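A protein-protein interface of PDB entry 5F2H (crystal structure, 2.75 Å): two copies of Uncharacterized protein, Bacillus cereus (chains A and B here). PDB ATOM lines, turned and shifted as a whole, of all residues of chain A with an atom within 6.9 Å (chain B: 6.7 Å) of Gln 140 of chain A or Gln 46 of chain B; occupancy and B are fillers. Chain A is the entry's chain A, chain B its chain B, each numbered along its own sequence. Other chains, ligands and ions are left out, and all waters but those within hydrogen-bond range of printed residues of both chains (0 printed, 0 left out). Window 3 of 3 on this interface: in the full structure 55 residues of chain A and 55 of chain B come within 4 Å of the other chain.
O of Ser 171 of chain A lies within hydrogen-bond range of ND2 of Asn 43 of chain B.
The backbone carbonyl oxygen (O) of Asp 172 of chain A lies within hydrogen-bond range of the side-chain amide nitrogen (ND2) of Asn 43 of chain B (2.9 Å).
The side-chain amide oxygen (OE1) of Gln 140 of chain A is in hydrogen-bond range of the side-chain amide nitrogen (NE2) of Gln 46 of chain B (2.9 Å).
The side-chain amide nitrogen (NE2) of Gln 140 of chain A sits close to the side-chain amide nitrogen (NE2) of Gln 169 of chain A.
N of Ala 45 of chain B sits at hydrogen-bond distance from OD1 of Asn 43 of chain B (3.0 Å).
The backbone carbonyl oxygen (O) of Asp 172 of chain A lies within hydrogen-bond range of the side-chain amide nitrogen (ND2) of Asn 142 of chain A (2.7 Å).
The side-chain amide oxygen (OD1) of Asn 142 of chain A lies within hydrogen-bond range of the backbone NH (N) of Ile 145 of chain A (3.0 Å).
O of Ala 45 of chain B lies within hydrogen-bond range of OH of Tyr 79 of chain B (2.5 Å).
N of Gln 140 of chain A is in hydrogen-bond range of O of Phe 174 of chain A (2.6 Å).
Ile 145 of chain A touches Tyr 10 of chain B (CD1 to CE2, 3.7 Å).
Asn 43 of chain B touches Phe 170 of chain A.
Phe 170 of chain A touches Tyr 79 of chain B.
Ser 171 of chain A touches Ala 45 of chain B.
CA of Phe 77 of chain B touches OG of Ser 171 of chain A, 3.1 Å away.
Asn 43 of chain B touches Gly 173 of chain A.
Gln 140 of chain A touches just one residue of chain B: Gln 46 (2.9 Å).
Gln 46 of chain B touches one residue of chain A.
Of the printed residues of chain B, Asp 172 of chain A touches Asn 43 (2.9 Å).
Printed residues of chain B within 4 Å of Ser 171 of chain A: Asn 43, Ala 45 and Phe 77.
Of the printed residues of chain B, Phe 170 of chain A touches Asn 43 and Tyr 79.
Of the printed residues of chain A, Asn 43 of chain B touches Phe 170 (3.5 Å), Ser 171 (3.3 Å), Asp 172 (2.9 Å) and Gly 173 (3.7 Å).
Ile 47 of chain B touches none of the printed residues of chain A.
The nearest residue of chain A that does not touch Gln 46 of chain B is Phe 170 of chain A (4.03 Å).
The nearest printed residue of chain A that does not touch Phe 77 of chain B is Asp 172 of chain A (4.6 Å).
Printed residues of chain B that touch a printed residue of chain A: Tyr 10, Asn 43, Ala 45, Gln 46, Phe 77 and Tyr 79.
Hydrophobic or aromatic side chains of chain B that line the printed part of chain A: Tyr 10, Ala 45, Phe 77 and Tyr 79.
Among the printed residues, 9 pairs touch across the chains.
No position is printed for both chains.
Of the 9 pairs that touch across the chains among the printed residues, none has its exchanged pair printed and touching as well.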
ATOM      1  N   HIS A 137     -17.910  22.367   2.722  1.00  0.00           N
ATOM      2  CA  HIS A 137     -18.681  23.273   1.870  1.00  0.00           C
ATOM      3  C   HIS A 137     -20.037  23.624   2.493  1.00  0.00           C
ATOM      4  O   HIS A 137     -20.523  22.925   3.411  1.00  0.00           O
ATOM      5  CB  HIS A 137     -18.932  22.638   0.515  1.00  0.00           C
ATOM      6  CG  HIS A 137     -19.824  21.446   0.558  1.00  0.00           C
ATOM      7  ND1 HIS A 137     -21.187  21.533   0.379  1.00  0.00           N
ATOM      8  CD2 HIS A 137     -19.555  20.130   0.738  1.00  0.00           C
ATOM      9  CE1 HIS A 137     -21.717  20.324   0.430  1.00  0.00           C
ATOM     10  NE2 HIS A 137     -20.749  19.454   0.650  1.00  0.00           N
ATOM     11  N   GLY A 138     -20.629  24.699   1.965  1.00  0.00           N
ATOM     12  CA  GLY A 138     -21.929  25.197   2.406  1.00  0.00           C
ATOM     13  C   GLY A 138     -23.078  24.542   1.677  1.00  0.00           C
ATOM     14  O   GLY A 138     -22.859  23.757   0.774  1.00  0.00           O
ATOM     15  N   ASP A 139     -24.309  24.831   2.059  1.00  0.00           N
ATOM     16  CA  ASP A 139     -25.403  24.214   1.365  1.00  0.00           C
ATOM     17  C   ASP A 139     -25.397  24.693  -0.074  1.00  0.00           C
ATOM     18  O   ASP A 139     -24.956  25.808  -0.366  1.00  0.00           O
ATOM     19  CB  ASP A 139     -26.747  24.502   2.023  1.00  0.00           C
ATOM     20  CG  ASP A 139     -26.950  23.726   3.332  1.00  0.00           C
ATOM     21  OD1 ASP A 139     -26.265  22.689   3.507  1.00  0.00           O
ATOM     22  OD2 ASP A 139     -27.841  24.118   4.148  1.00  0.00           O
ATOM     23  N   GLN A 140     -25.815  23.802  -0.970  1.00  0.00           N
ATOM     24  CA  GLN A 140     -25.912  24.097  -2.384  1.00  0.00           C
ATOM     25  C   GLN A 140     -24.568  24.350  -3.077  1.00  0.00           C
ATOM     26  O   GLN A 140     -24.493  25.050  -4.073  1.00  0.00           O
ATOM     27  CB  GLN A 140     -26.870  25.263  -2.595  1.00  0.00           C
ATOM     28  CG  GLN A 140     -28.248  24.950  -2.052  1.00  0.00           C
ATOM     29  CD  GLN A 140     -29.274  26.028  -2.271  1.00  0.00           C
ATOM     30  OE1 GLN A 140     -29.023  27.033  -2.940  1.00  0.00           O
ATOM     31  NE2 GLN A 140     -30.466  25.808  -1.726  1.00  0.00           N
ATOM     32  N   GLU A 141     -23.525  23.728  -2.542  1.00  0.00           N
ATOM     33  CA  GLU A 141     -22.205  23.843  -3.087  1.00  0.00           C
ATOM     34  C   GLU A 141     -21.686  22.456  -3.432  1.00  0.00           C
ATOM     35  O   GLU A 141     -22.454  21.514  -3.583  1.00  0.00           O
ATOM     36  CB  GLU A 141     -21.284  24.555  -2.095  1.00  0.00           C
ATOM     37  CG  GLU A 141     -21.653  25.998  -1.816  1.00  0.00           C
ATOM     38  CD  GLU A 141     -20.612  26.715  -0.977  1.00  0.00           C
ATOM     39  OE1 GLU A 141     -19.537  26.142  -0.706  1.00  0.00           O
ATOM     40  OE2 GLU A 141     -20.852  27.872  -0.589  1.00  0.00           O
ATOM     41  N   ASN A 142     -20.372  22.336  -3.548  1.00  0.00           N
ATOM     42  CA  ASN A 142     -19.725  21.093  -3.871  1.00  0.00           C
ATOM     43  C   ASN A 142     -18.228  21.300  -3.730  1.00  0.00           C
ATOM     44  O   ASN A 142     -17.797  22.331  -3.227  1.00  0.00           O
ATOM     45  CB  ASN A 142     -20.114  20.661  -5.288  1.00  0.00           C
ATOM     46  CG  ASN A 142     -19.793  21.717  -6.313  1.00  0.00           C
ATOM     47  OD1 ASN A 142     -18.774  22.383  -6.217  1.00  0.00           O
ATOM     48  ND2 ASN A 142     -20.663  21.869  -7.303  1.00  0.00           N
ATOM     49  N   ILE A 145     -16.584  24.407  -5.879  1.00  0.00           N
ATOM     50  CA  ILE A 145     -16.893  25.715  -5.310  1.00  0.00           C
ATOM     51  C   ILE A 145     -16.200  26.076  -4.012  1.00  0.00           C
ATOM     52  O   ILE A 145     -15.946  27.242  -3.743  1.00  0.00           O
ATOM     53  CB  ILE A 145     -18.405  25.813  -5.066  1.00  0.00           C
ATOM     54  CG1 ILE A 145     -19.139  25.762  -6.390  1.00  0.00           C
ATOM     55  CG2 ILE A 145     -18.751  27.109  -4.344  1.00  0.00           C
ATOM     56  CD1 ILE A 145     -20.638  25.737  -6.264  1.00  0.00           C
ATOM     57  N   GLN A 169     -29.517  18.124  -3.918  1.00  0.00           N
ATOM     58  CA  GLN A 169     -30.749  18.924  -4.071  1.00  0.00           C
ATOM     59  C   GLN A 169     -31.056  19.274  -5.533  1.00  0.00           C
ATOM     60  O   GLN A 169     -32.201  19.524  -5.880  1.00  0.00           O
ATOM     61  CB  GLN A 169     -30.596  20.211  -3.284  1.00  0.00           C
ATOM     62  CG  GLN A 169     -31.807  21.137  -3.298  1.00  0.00           C
ATOM     63  CD  GLN A 169     -31.493  22.458  -2.634  1.00  0.00           C
ATOM     64  OE1 GLN A 169     -30.599  22.549  -1.800  1.00  0.00           O
ATOM     65  NE2 GLN A 169     -32.199  23.501  -3.032  1.00  0.00           N
ATOM     66  N   PHE A 170     -30.012  19.369  -6.354  1.00  0.00           N
ATOM     67  CA  PHE A 170     -30.123  19.654  -7.774  1.00  0.00           C
ATOM     68  C   PHE A 170     -28.765  19.359  -8.371  1.00  0.00           C
ATOM     69  O   PHE A 170     -27.803  19.123  -7.632  1.00  0.00           O
ATOM     70  CB  PHE A 170     -30.538  21.081  -8.032  1.00  0.00           C
ATOM     71  CG  PHE A 170     -29.625  22.073  -7.433  1.00  0.00           C
ATOM     72  CD1 PHE A 170     -28.523  22.548  -8.148  1.00  0.00           C
ATOM     73  CD2 PHE A 170     -29.848  22.544  -6.160  1.00  0.00           C
ATOM     74  CE1 PHE A 170     -27.653  23.458  -7.585  1.00  0.00           C
ATOM     75  CE2 PHE A 170     -28.982  23.457  -5.590  1.00  0.00           C
ATOM     76  CZ  PHE A 170     -27.881  23.912  -6.305  1.00  0.00           C
ATOM     77  N   SER A 171     -28.693  19.324  -9.699  1.00  0.00           N
ATOM     78  CA  SER A 171     -27.444  19.045 -10.404  1.00  0.00           C
ATOM     79  C   SER A 171     -26.240  19.743  -9.783  1.00  0.00           C
ATOM     80  O   SER A 171     -26.195  20.962  -9.739  1.00  0.00           O
ATOM     81  CB  SER A 171     -27.546  19.479 -11.872  1.00  0.00           C
ATOM     82  OG  SER A 171     -28.547  18.763 -12.570  1.00  0.00           O
ATOM     83  N   ASP A 172     -25.277  18.958  -9.303  1.00  0.00           N
ATOM     84  CA  ASP A 172     -24.039  19.464  -8.699  1.00  0.00           C
ATOM     85  C   ASP A 172     -24.204  20.357  -7.459  1.00  0.00           C
ATOM     86  O   ASP A 172     -23.257  21.059  -7.091  1.00  0.00           O
ATOM     87  CB  ASP A 172     -23.212  20.228  -9.737  1.00  0.00           C
ATOM     88  CG  ASP A 172     -22.878  19.401 -10.940  1.00  0.00           C
ATOM     89  OD1 ASP A 172     -22.813  18.162 -10.813  1.00  0.00           O
ATOM     90  OD2 ASP A 172     -22.666  19.997 -12.021  1.00  0.00           O
ATOM     91  N   GLY A 173     -25.380  20.338  -6.828  1.00  0.00           N
ATOM     92  CA  GLY A 173     -25.649  21.142  -5.617  1.00  0.00           C
ATOM     93  C   GLY A 173     -25.898  20.189  -4.453  1.00  0.00           C
ATOM     94  O   GLY A 173     -26.836  19.387  -4.492  1.00  0.00           O
ATOM     95  N   PHE A 174     -25.105  20.302  -3.399  1.00  0.00           N
ATOM     96  CA  PHE A 174     -25.230  19.394  -2.261  1.00  0.00           C
ATOM     97  C   PHE A 174     -25.518  20.122  -0.920  1.00  0.00           C
ATOM     98  O   PHE A 174     -25.082  21.269  -0.742  1.00  0.00           O
ATOM     99  CB  PHE A 174     -23.944  18.570  -2.201  1.00  0.00           C
ATOM    100  CG  PHE A 174     -23.676  17.785  -3.454  1.00  0.00           C
ATOM    101  CD1 PHE A 174     -23.022  18.361  -4.523  1.00  0.00           C
ATOM    102  CD2 PHE A 174     -24.090  16.457  -3.565  1.00  0.00           C
ATOM    103  CE1 PHE A 174     -22.805  17.649  -5.683  1.00  0.00           C
ATOM    104  CE2 PHE A 174     -23.851  15.728  -4.719  1.00  0.00           C
ATOM    105  CZ  PHE A 174     -23.207  16.332  -5.777  1.00  0.00           C
ATOM    106  N   VAL A 175     -26.224  19.459  -0.001  1.00  0.00           N
ATOM    107  CA  VAL A 175     -26.591  20.070   1.285  1.00  0.00           C
ATOM    108  C   VAL A 175     -26.415  19.227   2.540  1.00  0.00           C
ATOM    109  O   VAL A 175     -26.424  17.999   2.496  1.00  0.00           O
ATOM    110  CB  VAL A 175     -28.083  20.450   1.332  1.00  0.00           C
ATOM    111  CG1 VAL A 175     -28.413  21.495   0.271  1.00  0.00           C
ATOM    112  CG2 VAL A 175     -28.973  19.219   1.175  1.00  0.00           C
ATOM    113  N   TRP A 176     -26.332  19.928   3.668  1.00  0.00           N
ATOM    114  CA  TRP A 176     -26.174  19.302   4.986  1.00  0.00           C
ATOM    115  C   TRP A 176     -27.451  19.330   5.839  1.00  0.00           C
ATOM    116  O   TRP A 176     -27.379  19.442   7.042  1.00  0.00           O
ATOM    117  CB  TRP A 176     -25.061  19.992   5.752  1.00  0.00           C
ATOM    118  CG  TRP A 176     -23.761  19.948   5.048  1.00  0.00           C
ATOM    119  CD1 TRP A 176     -23.161  20.952   4.366  1.00  0.00           C
ATOM    120  CD2 TRP A 176     -22.923  18.802   4.905  1.00  0.00           C
ATOM    121  NE1 TRP A 176     -21.979  20.516   3.830  1.00  0.00           N
ATOM    122  CE2 TRP A 176     -21.805  19.199   4.156  1.00  0.00           C
ATOM    123  CE3 TRP A 176     -23.004  17.480   5.360  1.00  0.00           C
ATOM    124  CZ2 TRP A 176     -20.773  18.335   3.843  1.00  0.00           C
ATOM    125  CZ3 TRP A 176     -21.959  16.626   5.073  1.00  0.00           C
ATOM    126  CH2 TRP A 176     -20.857  17.062   4.302  1.00  0.00           C
ATOM    127  N   TYR B  10     -18.340  33.294  -8.011  1.00  0.00           N
ATOM    128  CA  TYR B  10     -19.654  32.674  -8.093  1.00  0.00           C
ATOM    129  C   TYR B  10     -20.532  33.186  -6.955  1.00  0.00           C
ATOM    130  O   TYR B  10     -21.659  33.643  -7.161  1.00  0.00           O
ATOM    131  CB  TYR B  10     -19.464  31.178  -8.013  1.00  0.00           C
ATOM    132  CG  TYR B  10     -20.719  30.370  -7.897  1.00  0.00           C
ATOM    133  CD1 TYR B  10     -21.432  30.000  -9.019  1.00  0.00           C
ATOM    134  CD2 TYR B  10     -21.136  29.882  -6.656  1.00  0.00           C
ATOM    135  CE1 TYR B  10     -22.560  29.216  -8.912  1.00  0.00           C
ATOM    136  CE2 TYR B  10     -22.258  29.099  -6.547  1.00  0.00           C
ATOM    137  CZ  TYR B  10     -22.969  28.776  -7.679  1.00  0.00           C
ATOM    138  OH  TYR B  10     -24.076  27.984  -7.576  1.00  0.00           O
ATOM    139  N   LEU B  14     -23.915  35.611  -7.096  1.00  0.00           N
ATOM    140  CA  LEU B  14     -25.178  35.195  -6.448  1.00  0.00           C
ATOM    141  C   LEU B  14     -25.675  36.150  -5.364  1.00  0.00           C
ATOM    142  O   LEU B  14     -26.859  36.483  -5.340  1.00  0.00           O
ATOM    143  CB  LEU B  14     -25.100  33.751  -5.927  1.00  0.00           C
ATOM    144  CG  LEU B  14     -24.878  32.669  -7.007  1.00  0.00           C
ATOM    145  CD1 LEU B  14     -24.727  31.319  -6.363  1.00  0.00           C
ATOM    146  CD2 LEU B  14     -25.992  32.606  -8.034  1.00  0.00           C
ATOM    147  N   ILE B  33     -27.889  39.794 -13.388  1.00  0.00           N
ATOM    148  CA  ILE B  33     -27.233  38.511 -13.578  1.00  0.00           C
ATOM    149  C   ILE B  33     -26.923  38.220 -15.042  1.00  0.00           C
ATOM    150  O   ILE B  33     -25.925  37.558 -15.323  1.00  0.00           O
ATOM    151  CB  ILE B  33     -28.048  37.351 -12.969  1.00  0.00           C
ATOM    152  CG1 ILE B  33     -27.199  36.077 -12.872  1.00  0.00           C
ATOM    153  CG2 ILE B  33     -29.331  37.119 -13.742  1.00  0.00           C
ATOM    154  CD1 ILE B  33     -27.875  34.948 -12.123  1.00  0.00           C
ATOM    155  N   ASN B  43     -21.340  26.657 -10.690  1.00  0.00           N
ATOM    156  CA  ASN B  43     -22.412  25.665 -10.799  1.00  0.00           C
ATOM    157  C   ASN B  43     -23.402  26.339 -11.716  1.00  0.00           C
ATOM    158  O   ASN B  43     -24.114  27.244 -11.311  1.00  0.00           O
ATOM    159  CB  ASN B  43     -23.046  25.301  -9.449  1.00  0.00           C
ATOM    160  CG  ASN B  43     -24.120  24.218  -9.575  1.00  0.00           C
ATOM    161  OD1 ASN B  43     -24.837  24.133 -10.575  1.00  0.00           O
ATOM    162  ND2 ASN B  43     -24.260  23.414  -8.539  1.00  0.00           N
ATOM    163  N   GLU B  44     -23.409  25.914 -12.969  1.00  0.00           N
ATOM    164  CA  GLU B  44     -24.296  26.507 -13.940  1.00  0.00           C
ATOM    165  C   GLU B  44     -25.751  26.275 -13.618  1.00  0.00           C
ATOM    166  O   GLU B  44     -26.576  27.162 -13.788  1.00  0.00           O
ATOM    167  CB  GLU B  44     -23.998  25.985 -15.341  1.00  0.00           C
ATOM    168  CG  GLU B  44     -22.638  26.357 -15.884  1.00  0.00           C
ATOM    169  CD  GLU B  44     -22.513  25.927 -17.327  1.00  0.00           C
ATOM    170  OE1 GLU B  44     -23.317  25.071 -17.741  1.00  0.00           O
ATOM    171  OE2 GLU B  44     -21.626  26.433 -18.054  1.00  0.00           O
ATOM    172  N   ALA B  45     -26.064  25.057 -13.197  1.00  0.00           N
ATOM    173  CA  ALA B  45     -27.430  24.694 -12.856  1.00  0.00           C
ATOM    174  C   ALA B  45     -28.018  25.761 -11.958  1.00  0.00           C
ATOM    175  O   ALA B  45     -29.080  26.285 -12.230  1.00  0.00           O
ATOM    176  CB  ALA B  45     -27.455  23.339 -12.176  1.00  0.00           C
ATOM    177  N   GLN B  46     -27.282  26.119 -10.919  1.00  0.00           N
ATOM    178  CA  GLN B  46     -27.699  27.143  -9.985  1.00  0.00           C
ATOM    179  C   GLN B  46     -27.825  28.495 -10.661  1.00  0.00           C
ATOM    180  O   GLN B  46     -28.717  29.277 -10.331  1.00  0.00           O
ATOM    181  CB  GLN B  46     -26.670  27.231  -8.866  1.00  0.00           C
ATOM    182  CG  GLN B  46     -26.998  28.204  -7.731  1.00  0.00           C
ATOM    183  CD  GLN B  46     -28.280  27.867  -6.972  1.00  0.00           C
ATOM    184  OE1 GLN B  46     -29.343  27.707  -7.568  1.00  0.00           O
ATOM    185  NE2 GLN B  46     -28.200  27.885  -5.641  1.00  0.00           N
ATOM    186  N   ILE B  47     -26.914  28.786 -11.596  1.00  0.00           N
ATOM    187  CA  ILE B  47     -26.957  30.048 -12.341  1.00  0.00           C
ATOM    188  C   ILE B  47     -28.199  30.082 -13.231  1.00  0.00           C
ATOM    189  O   ILE B  47     -28.880  31.112 -13.311  1.00  0.00           O
ATOM    190  CB  ILE B  47     -25.683  30.276 -13.153  1.00  0.00           C
ATOM    191  CG1 ILE B  47     -24.500  30.442 -12.201  1.00  0.00           C
ATOM    192  CG2 ILE B  47     -25.790  31.541 -13.991  1.00  0.00           C
ATOM    193  CD1 ILE B  47     -23.168  30.533 -12.906  1.00  0.00           C
ATOM    194  N   TYR B  48     -28.510  28.978 -13.899  1.00  0.00           N
ATOM    195  CA  TYR B  48     -29.713  28.947 -14.737  1.00  0.00           C
ATOM    196  C   TYR B  48     -30.975  29.074 -13.922  1.00  0.00           C
ATOM    197  O   TYR B  48     -31.918  29.728 -14.360  1.00  0.00           O
ATOM    198  CB  TYR B  48     -29.823  27.687 -15.602  1.00  0.00           C
ATOM    199  CG  TYR B  48     -28.907  27.668 -16.802  1.00  0.00           C
ATOM    200  CD1 TYR B  48     -29.267  28.326 -17.966  1.00  0.00           C
ATOM    201  CD2 TYR B  48     -27.724  26.951 -16.799  1.00  0.00           C
ATOM    202  CE1 TYR B  48     -28.463  28.296 -19.083  1.00  0.00           C
ATOM    203  CE2 TYR B  48     -26.904  26.919 -17.915  1.00  0.00           C
ATOM    204  CZ  TYR B  48     -27.283  27.585 -19.056  1.00  0.00           C
ATOM    205  OH  TYR B  48     -26.483  27.565 -20.173  1.00  0.00           O
ATOM    206  N   ASN B  49     -31.014  28.424 -12.759  1.00  0.00           N
ATOM    207  CA  ASN B  49     -32.190  28.479 -11.927  1.00  0.00           C
ATOM    208  C   ASN B  49     -32.426  29.935 -11.655  1.00  0.00           C
ATOM    209  O   ASN B  49     -33.514  30.441 -11.922  1.00  0.00           O
ATOM    210  CB  ASN B  49     -32.016  27.678 -10.642  1.00  0.00           C
ATOM    211  CG  ASN B  49     -33.276  27.640  -9.798  1.00  0.00           C
ATOM    212  OD1 ASN B  49     -34.363  28.015 -10.242  1.00  0.00           O
ATOM    213  ND2 ASN B  49     -33.144  27.140  -8.586  1.00  0.00           N
ATOM    214  N   PHE B  50     -31.403  30.635 -11.171  1.00  0.00           N
ATOM    215  CA  PHE B  50     -31.562  32.077 -10.917  1.00  0.00           C
ATOM    216  C   PHE B  50     -32.090  32.832 -12.132  1.00  0.00           C
ATOM    217  O   PHE B  50     -33.045  33.612 -12.016  1.00  0.00           O
ATOM    218  CB  PHE B  50     -30.279  32.714 -10.406  1.00  0.00           C
ATOM    219  CG  PHE B  50     -30.068  32.567  -8.918  1.00  0.00           C
ATOM    220  CD1 PHE B  50     -29.742  31.346  -8.345  1.00  0.00           C
ATOM    221  CD2 PHE B  50     -30.102  33.684  -8.102  1.00  0.00           C
ATOM    222  CE1 PHE B  50     -29.547  31.229  -6.973  1.00  0.00           C
ATOM    223  CE2 PHE B  50     -29.887  33.573  -6.738  1.00  0.00           C
ATOM    224  CZ  PHE B  50     -29.618  32.340  -6.171  1.00  0.00           C
ATOM    225  N   LYS B  51     -31.531  32.553 -13.301  1.00  0.00           N
ATOM    226  CA  LYS B  51     -31.980  33.247 -14.506  1.00  0.00           C
ATOM    227  C   LYS B  51     -33.455  33.065 -14.852  1.00  0.00           C
ATOM    228  O   LYS B  51     -34.189  34.049 -14.946  1.00  0.00           O
ATOM    229  CB  LYS B  51     -31.105  32.920 -15.721  1.00  0.00           C
ATOM    230  CG  LYS B  51     -29.694  33.463 -15.624  1.00  0.00           C
ATOM    231  CD  LYS B  51     -28.875  33.142 -16.857  1.00  0.00           C
ATOM    232  CE  LYS B  51     -27.472  33.729 -16.720  1.00  0.00           C
ATOM    233  NZ  LYS B  51     -26.626  33.569 -17.936  1.00  0.00           N
ATOM    234  N   PHE B  77     -29.569  19.392 -16.895  1.00  0.00           N
ATOM    235  CA  PHE B  77     -29.592  19.514 -15.443  1.00  0.00           C
ATOM    236  C   PHE B  77     -30.998  19.224 -14.937  1.00  0.00           C
ATOM    237  O   PHE B  77     -31.931  19.085 -15.730  1.00  0.00           O
ATOM    238  CB  PHE B  77     -29.234  20.917 -14.971  1.00  0.00           C
ATOM    239  CG  PHE B  77     -27.904  21.414 -15.448  1.00  0.00           C
ATOM    240  CD1 PHE B  77     -26.736  20.769 -15.075  1.00  0.00           C
ATOM    241  CD2 PHE B  77     -27.813  22.638 -16.087  1.00  0.00           C
ATOM    242  CE1 PHE B  77     -25.505  21.271 -15.437  1.00  0.00           C
ATOM    243  CE2 PHE B  77     -26.592  23.143 -16.459  1.00  0.00           C
ATOM    244  CZ  PHE B  77     -25.433  22.460 -16.137  1.00  0.00           C
ATOM    245  N   TYR B  79     -33.838  19.929 -11.269  1.00  0.00           N
ATOM    246  CA  TYR B  79     -34.112  20.633 -10.016  1.00  0.00           C
ATOM    247  C   TYR B  79     -35.206  19.914  -9.233  1.00  0.00           C
ATOM    248  O   TYR B  79     -35.948  19.107  -9.790  1.00  0.00           O
ATOM    249  CB  TYR B  79     -34.529  22.060 -10.301  1.00  0.00           C
ATOM    250  CG  TYR B  79     -33.504  22.797 -11.137  1.00  0.00           C
ATOM    251  CD1 TYR B  79     -32.427  23.424 -10.547  1.00  0.00           C
ATOM    252  CD2 TYR B  79     -33.603  22.840 -12.513  1.00  0.00           C
ATOM    253  CE1 TYR B  79     -31.478  24.079 -11.307  1.00  0.00           C
ATOM    254  CE2 TYR B  79     -32.672  23.508 -13.272  1.00  0.00           C
ATOM    255  CZ  TYR B  79     -31.609  24.132 -12.664  1.00  0.00           C
ATOM    256  OH  TYR B  79     -30.675  24.804 -13.435  1.00  0.00           O
